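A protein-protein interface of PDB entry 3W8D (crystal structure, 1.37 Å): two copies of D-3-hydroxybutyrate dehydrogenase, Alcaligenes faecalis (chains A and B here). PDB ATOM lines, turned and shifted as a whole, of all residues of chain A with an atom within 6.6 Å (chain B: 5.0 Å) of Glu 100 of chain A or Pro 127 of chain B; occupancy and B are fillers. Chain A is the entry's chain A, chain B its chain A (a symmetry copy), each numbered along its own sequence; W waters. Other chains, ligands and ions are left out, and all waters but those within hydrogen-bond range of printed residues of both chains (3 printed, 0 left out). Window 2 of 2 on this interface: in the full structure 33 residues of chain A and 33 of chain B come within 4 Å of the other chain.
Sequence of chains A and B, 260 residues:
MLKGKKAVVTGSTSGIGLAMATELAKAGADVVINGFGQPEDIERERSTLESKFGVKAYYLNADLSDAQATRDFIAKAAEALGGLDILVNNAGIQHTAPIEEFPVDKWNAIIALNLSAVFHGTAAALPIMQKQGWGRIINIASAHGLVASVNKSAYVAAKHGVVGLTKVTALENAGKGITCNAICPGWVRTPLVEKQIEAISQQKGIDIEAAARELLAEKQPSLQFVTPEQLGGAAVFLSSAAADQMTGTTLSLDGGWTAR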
ATOM      1  N   ALA A  97      10.950 -35.153 -32.144  1.00  0.00           N
ATOM      2  CA  ALA A  97      11.007 -33.936 -31.265  1.00  0.00           C
ATOM      3  C   ALA A  97      12.299 -33.251 -31.590  1.00  0.00           C
ATOM      4  O   ALA A  97      13.290 -33.933 -31.924  1.00  0.00           O
ATOM      5  CB  ALA A  97      11.071 -34.325 -29.756  1.00  0.00           C
ATOM      6  N   PRO A  98      12.397 -31.954 -31.381  1.00  0.00           N
ATOM      7  CA  PRO A  98      13.704 -31.244 -31.552  1.00  0.00           C
ATOM      8  C   PRO A  98      14.673 -31.749 -30.474  1.00  0.00           C
ATOM      9  O   PRO A  98      14.246 -32.200 -29.361  1.00  0.00           O
ATOM     10  CB  PRO A  98      13.416 -29.773 -31.288  1.00  0.00           C
ATOM     11  CG  PRO A  98      12.038 -29.729 -30.899  1.00  0.00           C
ATOM     12  CD  PRO A  98      11.314 -31.030 -31.076  1.00  0.00           C
ATOM     13  N   ILE A  99      15.964 -31.614 -30.697  1.00  0.00           N
ATOM     14  CA  ILE A  99      16.978 -32.184 -29.771  1.00  0.00           C
ATOM     15  C   ILE A  99      16.765 -31.742 -28.336  1.00  0.00           C
ATOM     16  O   ILE A  99      16.860 -32.588 -27.406  1.00  0.00           O
ATOM     17  CB  ILE A  99      18.397 -31.796 -30.281  1.00  0.00           C
ATOM     18  CG1 ILE A  99      18.709 -32.621 -31.533  1.00  0.00           C
ATOM     19  CG2 ILE A  99      19.432 -32.146 -29.168  1.00  0.00           C
ATOM     20  CD1 ILE A  99      19.923 -32.078 -32.380  1.00  0.00           C
ATOM     21  N   GLU A 100      16.625 -30.456 -28.102  1.00  0.00           N
ATOM     22  CA  GLU A 100      16.565 -29.963 -26.702  1.00  0.00           C
ATOM     23  C   GLU A 100      15.278 -30.442 -26.040  1.00  0.00           C
ATOM     24  O   GLU A 100      15.162 -30.255 -24.809  1.00  0.00           O
ATOM     25  CB  GLU A 100      16.686 -28.449 -26.695  1.00  0.00           C
ATOM     26  CG  GLU A 100      15.545 -27.638 -27.380  1.00  0.00           C
ATOM     27  CD  GLU A 100      15.640 -27.494 -28.884  1.00  0.00           C
ATOM     28  OE1 GLU A 100      16.550 -28.070 -29.484  1.00  0.00           O
ATOM     29  OE2 GLU A 100      14.847 -26.777 -29.514  1.00  0.00           O
ATOM     30  N   GLU A 101      14.262 -30.941 -26.729  1.00  0.00           N
ATOM     31  CA  GLU A 101      13.051 -31.450 -26.146  1.00  0.00           C
ATOM     32  C   GLU A 101      13.026 -32.991 -26.262  1.00  0.00           C
ATOM     33  O   GLU A 101      12.008 -33.643 -25.928  1.00  0.00           O
ATOM     34  CB  GLU A 101      11.786 -30.915 -26.895  1.00  0.00           C
ATOM     35  CG  GLU A 101      11.644 -29.454 -26.663  1.00  0.00           C
ATOM     36  CD  GLU A 101      10.620 -28.757 -27.653  1.00  0.00           C
ATOM     37  OE1 GLU A 101       9.839 -29.421 -28.346  1.00  0.00           O
ATOM     38  OE2 GLU A 101      10.654 -27.518 -27.818  1.00  0.00           O
ATOM     39  N   PHE A 102      14.061 -33.625 -26.789  1.00  0.00           N
ATOM     40  CA  PHE A 102      13.948 -35.018 -27.124  1.00  0.00           C
ATOM     41  C   PHE A 102      14.096 -35.869 -25.865  1.00  0.00           C
ATOM     42  O   PHE A 102      15.133 -35.796 -25.185  1.00  0.00           O
ATOM     43  CB  PHE A 102      15.105 -35.367 -28.154  1.00  0.00           C
ATOM     44  CG  PHE A 102      14.785 -36.643 -28.924  1.00  0.00           C
ATOM     45  CD1 PHE A 102      14.258 -36.548 -30.231  1.00  0.00           C
ATOM     46  CD2 PHE A 102      14.947 -37.913 -28.358  1.00  0.00           C
ATOM     47  CE1 PHE A 102      13.900 -37.735 -30.964  1.00  0.00           C
ATOM     48  CE2 PHE A 102      14.642 -39.058 -29.034  1.00  0.00           C
ATOM     49  CZ  PHE A 102      14.095 -38.970 -30.365  1.00  0.00           C
ATOM     50  N   THR B 122      24.884 -31.403 -26.536  1.00  0.00           N
ATOM     51  CA  THR B 122      24.165 -30.562 -27.506  1.00  0.00           C
ATOM     52  C   THR B 122      22.785 -30.110 -26.970  1.00  0.00           C
ATOM     53  O   THR B 122      22.401 -28.949 -27.110  1.00  0.00           O
ATOM     54  CB  THR B 122      24.047 -31.405 -28.836  1.00  0.00           C
ATOM     55  OG1 THR B 122      25.357 -31.620 -29.371  1.00  0.00           O
ATOM     56  CG2 THR B 122      23.230 -30.560 -29.886  1.00  0.00           C
ATOM     57  N   ALA B 123      22.033 -31.075 -26.470  1.00  0.00           N
ATOM     58  CA  ALA B 123      20.689 -30.705 -25.936  1.00  0.00           C
ATOM     59  C   ALA B 123      20.762 -29.669 -24.848  1.00  0.00           C
ATOM     60  O   ALA B 123      19.945 -28.786 -24.822  1.00  0.00           O
ATOM     61  CB  ALA B 123      20.048 -31.994 -25.389  1.00  0.00           C
ATOM     62  N   ALA B 124      21.781 -29.793 -23.973  1.00  0.00           N
ATOM     63  CA  ALA B 124      21.857 -28.813 -22.870  1.00  0.00           C
ATOM     64  C   ALA B 124      22.378 -27.471 -23.370  1.00  0.00           C
ATOM     65  O   ALA B 124      22.037 -26.418 -22.850  1.00  0.00           O
ATOM     66  CB  ALA B 124      22.764 -29.332 -21.781  1.00  0.00           C
ATOM     67  N   ALA B 125      23.232 -27.454 -24.392  1.00  0.00           N
ATOM     68  CA  ALA B 125      23.784 -26.193 -24.869  1.00  0.00           C
ATOM     69  C   ALA B 125      22.846 -25.379 -25.747  1.00  0.00           C
ATOM     70  O   ALA B 125      22.941 -24.193 -25.840  1.00  0.00           O
ATOM     71  CB  ALA B 125      25.143 -26.399 -25.615  1.00  0.00           C
ATOM     72  N   LEU B 126      22.036 -26.140 -26.537  1.00  0.00           N
ATOM     73  CA  LEU B 126      21.234 -25.466 -27.544  1.00  0.00           C
ATOM     74  C   LEU B 126      20.379 -24.278 -27.064  1.00  0.00           C
ATOM     75  O   LEU B 126      20.337 -23.312 -27.771  1.00  0.00           O
ATOM     76  CB  LEU B 126      20.419 -26.507 -28.351  1.00  0.00           C
ATOM     77  CG  LEU B 126      21.186 -27.188 -29.527  1.00  0.00           C
ATOM     78  CD1 LEU B 126      20.333 -28.380 -30.061  1.00  0.00           C
ATOM     79  CD2 LEU B 126      21.482 -26.128 -30.654  1.00  0.00           C
ATOM     80  N   PRO B 127      19.652 -24.418 -25.917  1.00  0.00           N
ATOM     81  CA  PRO B 127      18.745 -23.321 -25.580  1.00  0.00           C
ATOM     82  C   PRO B 127      19.552 -22.020 -25.301  1.00  0.00           C
ATOM     83  O   PRO B 127      19.062 -20.923 -25.587  1.00  0.00           O
ATOM     84  CB  PRO B 127      18.061 -23.868 -24.335  1.00  0.00           C
ATOM     85  CG  PRO B 127      18.002 -25.411 -24.611  1.00  0.00           C
ATOM     86  CD  PRO B 127      19.388 -25.663 -25.194  1.00  0.00           C
ATOM     87  N   ILE B 128      20.792 -22.173 -24.802  1.00  0.00           N
ATOM     88  CA  ILE B 128      21.638 -20.993 -24.512  1.00  0.00           C
ATOM     89  C   ILE B 128      22.016 -20.318 -25.811  1.00  0.00           C
ATOM     90  O   ILE B 128      21.868 -19.091 -26.040  1.00  0.00           O
ATOM     91  CB  ILE B 128      22.880 -21.469 -23.747  1.00  0.00           C
ATOM     92  CG1 ILE B 128      22.453 -22.136 -22.424  1.00  0.00           C
ATOM     93  CG2 ILE B 128      23.898 -20.243 -23.590  1.00  0.00           C
ATOM     94  CD1 ILE B 128      23.628 -22.866 -21.699  1.00  0.00           C
ATOM     95  N   MET B 129      22.405 -21.131 -26.834  1.00  0.00           N
ATOM     96  CA  MET B 129      22.737 -20.614 -28.154  1.00  0.00           C
ATOM     97  C   MET B 129      21.537 -20.041 -28.904  1.00  0.00           C
ATOM     98  O   MET B 129      21.618 -18.997 -29.559  1.00  0.00           O
ATOM     99  CB  MET B 129      23.427 -21.737 -29.007  1.00  0.00           C
ATOM    100  CG  MET B 129      24.744 -22.172 -28.285  1.00  0.00           C
ATOM    101  SD  MET B 129      25.412 -23.502 -29.354  1.00  0.00           S
ATOM    102  CE  MET B 129      27.020 -23.762 -28.445  1.00  0.00           C
ATOM    103  N   GLN B 130      20.398 -20.736 -28.740  1.00  0.00           N
ATOM    104  CA  GLN B 130      19.140 -20.230 -29.411  1.00  0.00           C
ATOM    105  C   GLN B 130      18.693 -18.908 -28.867  1.00  0.00           C
ATOM    106  O   GLN B 130      18.347 -18.019 -29.660  1.00  0.00           O
ATOM    107  CB  GLN B 130      18.078 -21.298 -29.238  1.00  0.00           C
ATOM    108  CG  GLN B 130      18.355 -22.628 -30.061  1.00  0.00           C
ATOM    109  CD  GLN B 130      17.511 -23.795 -29.657  1.00  0.00           C
ATOM    110  OE1 GLN B 130      17.389 -24.772 -30.436  1.00  0.00           O
ATOM    111  NE2 GLN B 130      16.968 -23.822 -28.432  1.00  0.00           N
ATOM    112  N   LYS B 131      18.816 -18.729 -27.565  1.00  0.00           N
ATOM    113  CA  LYS B 131      18.342 -17.436 -26.985  1.00  0.00           C
ATOM    114  C   LYS B 131      19.288 -16.348 -27.429  1.00  0.00           C
ATOM    115  O   LYS B 131      18.793 -15.208 -27.590  1.00  0.00           O
ATOM    116  CB  LYS B 131      18.419 -17.569 -25.456  1.00  0.00           C
ATOM    117  CG  LYS B 131      18.011 -16.327 -24.668  1.00  0.00           C
ATOM    118  CD  LYS B 131      18.445 -16.352 -23.134  1.00  0.00           C
ATOM    119  CE  LYS B 131      19.080 -14.941 -22.711  1.00  0.00           C
ATOM    120  NZ  LYS B 131      18.884 -14.539 -21.258  1.00  0.00           N
ATOM    121  N   GLU B 172      17.960 -28.480 -37.597  1.00  0.00           N
ATOM    122  CA  GLU B 172      17.022 -27.955 -36.616  1.00  0.00           C
ATOM    123  C   GLU B 172      17.338 -26.527 -36.284  1.00  0.00           C
ATOM    124  O   GLU B 172      16.417 -25.825 -35.809  1.00  0.00           O
ATOM    125  CB  GLU B 172      17.093 -28.805 -35.335  1.00  0.00           C
ATOM    126  CG  GLU B 172      16.436 -30.197 -35.519  1.00  0.00           C
ATOM    127  CD  GLU B 172      16.404 -31.041 -34.243  1.00  0.00           C
ATOM    128  OE1 GLU B 172      16.696 -30.461 -33.153  1.00  0.00           O
ATOM    129  OE2 GLU B 172      16.011 -32.209 -34.350  1.00  0.00           O
HETATM  130  O   HOH W   1      15.203 -26.427 -32.535  1.00  0.00           O
HETATM  131  O   HOH W   2      17.326 -28.065 -32.111  1.00  0.00           O
HETATM  132  O   HOH W   3      15.845 -34.402 -32.807  1.00  0.00           O
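The side-chain carboxylate of Glu 172 of chain B sits at hydrogen-bond distance from the backbone NH of Ile 99 of chain A, at 2.8 Å. The side-chain amide oxygen (OE1) of Gln 130 of chain B sits close to the side-chain carboxylate (OE2) of Glu 100 of chain A (3.4 Å).
NE2 of Gln 130 of chain B sits close to O of Leu 126 of chain B (3.5 Å).
Among the printed residues, pairs that only touch across the chains: Pro 98 of chain A with Glu 172 of chain B (3.5 Å), Ile 99 of chain A with Ala 123 of chain B (3.8 Å), Glu 100 of chain A with Ala 123 of chain B (3.8 Å), Glu 100 of chain A with Leu 126 of chain B (3.8 Å), Glu 100 of chain A with Pro 127 of chain B (3.9 Å) and Ile 99 of chain A with Leu 126 of chain B (3.9 Å).
Of the printed residues of chain B, Pro 98 of chain A touches Glu 172. Of the printed residues of chain B, Glu 100 of chain A touches Ala 123, Leu 126, Pro 127 and Gln 130. Printed residues of chain A within 4 Å of Leu 126 of chain B: Ile 99 (3.9 Å) and Glu 100 (3.8 Å). Pro 127 of chain B touches one residue of chain A. Ile 128 of chain B touches none of the printed residues of chain A. Of the printed residues of chain A, Gln 130 of chain B touches Glu 100.
Of the 11 printed residues of chain B, 5 touch a printed residue of chain A. Hydrophobic or aromatic side chains of chain B within 4 Å of the printed part of chain A: Ala 123, Leu 126 and Pro 127. Of the 6 printed residues of chain A, 3 touch a printed residue of chain B. Along chain A the printed residues that touch a printed residue of chain B span positions 98 to 100.
No position is printed for both chains.
Water W3 lies within hydrogen-bond range of OE2 of Glu 172 of chain B (2.7 Å), O of Ala 97 of chain A (2.7 Å) and N of Ile 99 of chain A (3.5 Å). Water W2 lies within hydrogen-bond range of the side-chain carboxylate (OE1) of Glu 172 of chain B (2.7 Å) and the side-chain carboxylate (OE1) of Glu 100 of chain A (2.7 Å). Water W1 lies within hydrogen-bond range of OE2 of Glu 100 of chain A (3.1 Å) and OE1 of Gln 130 of chain B (3.5 Å).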
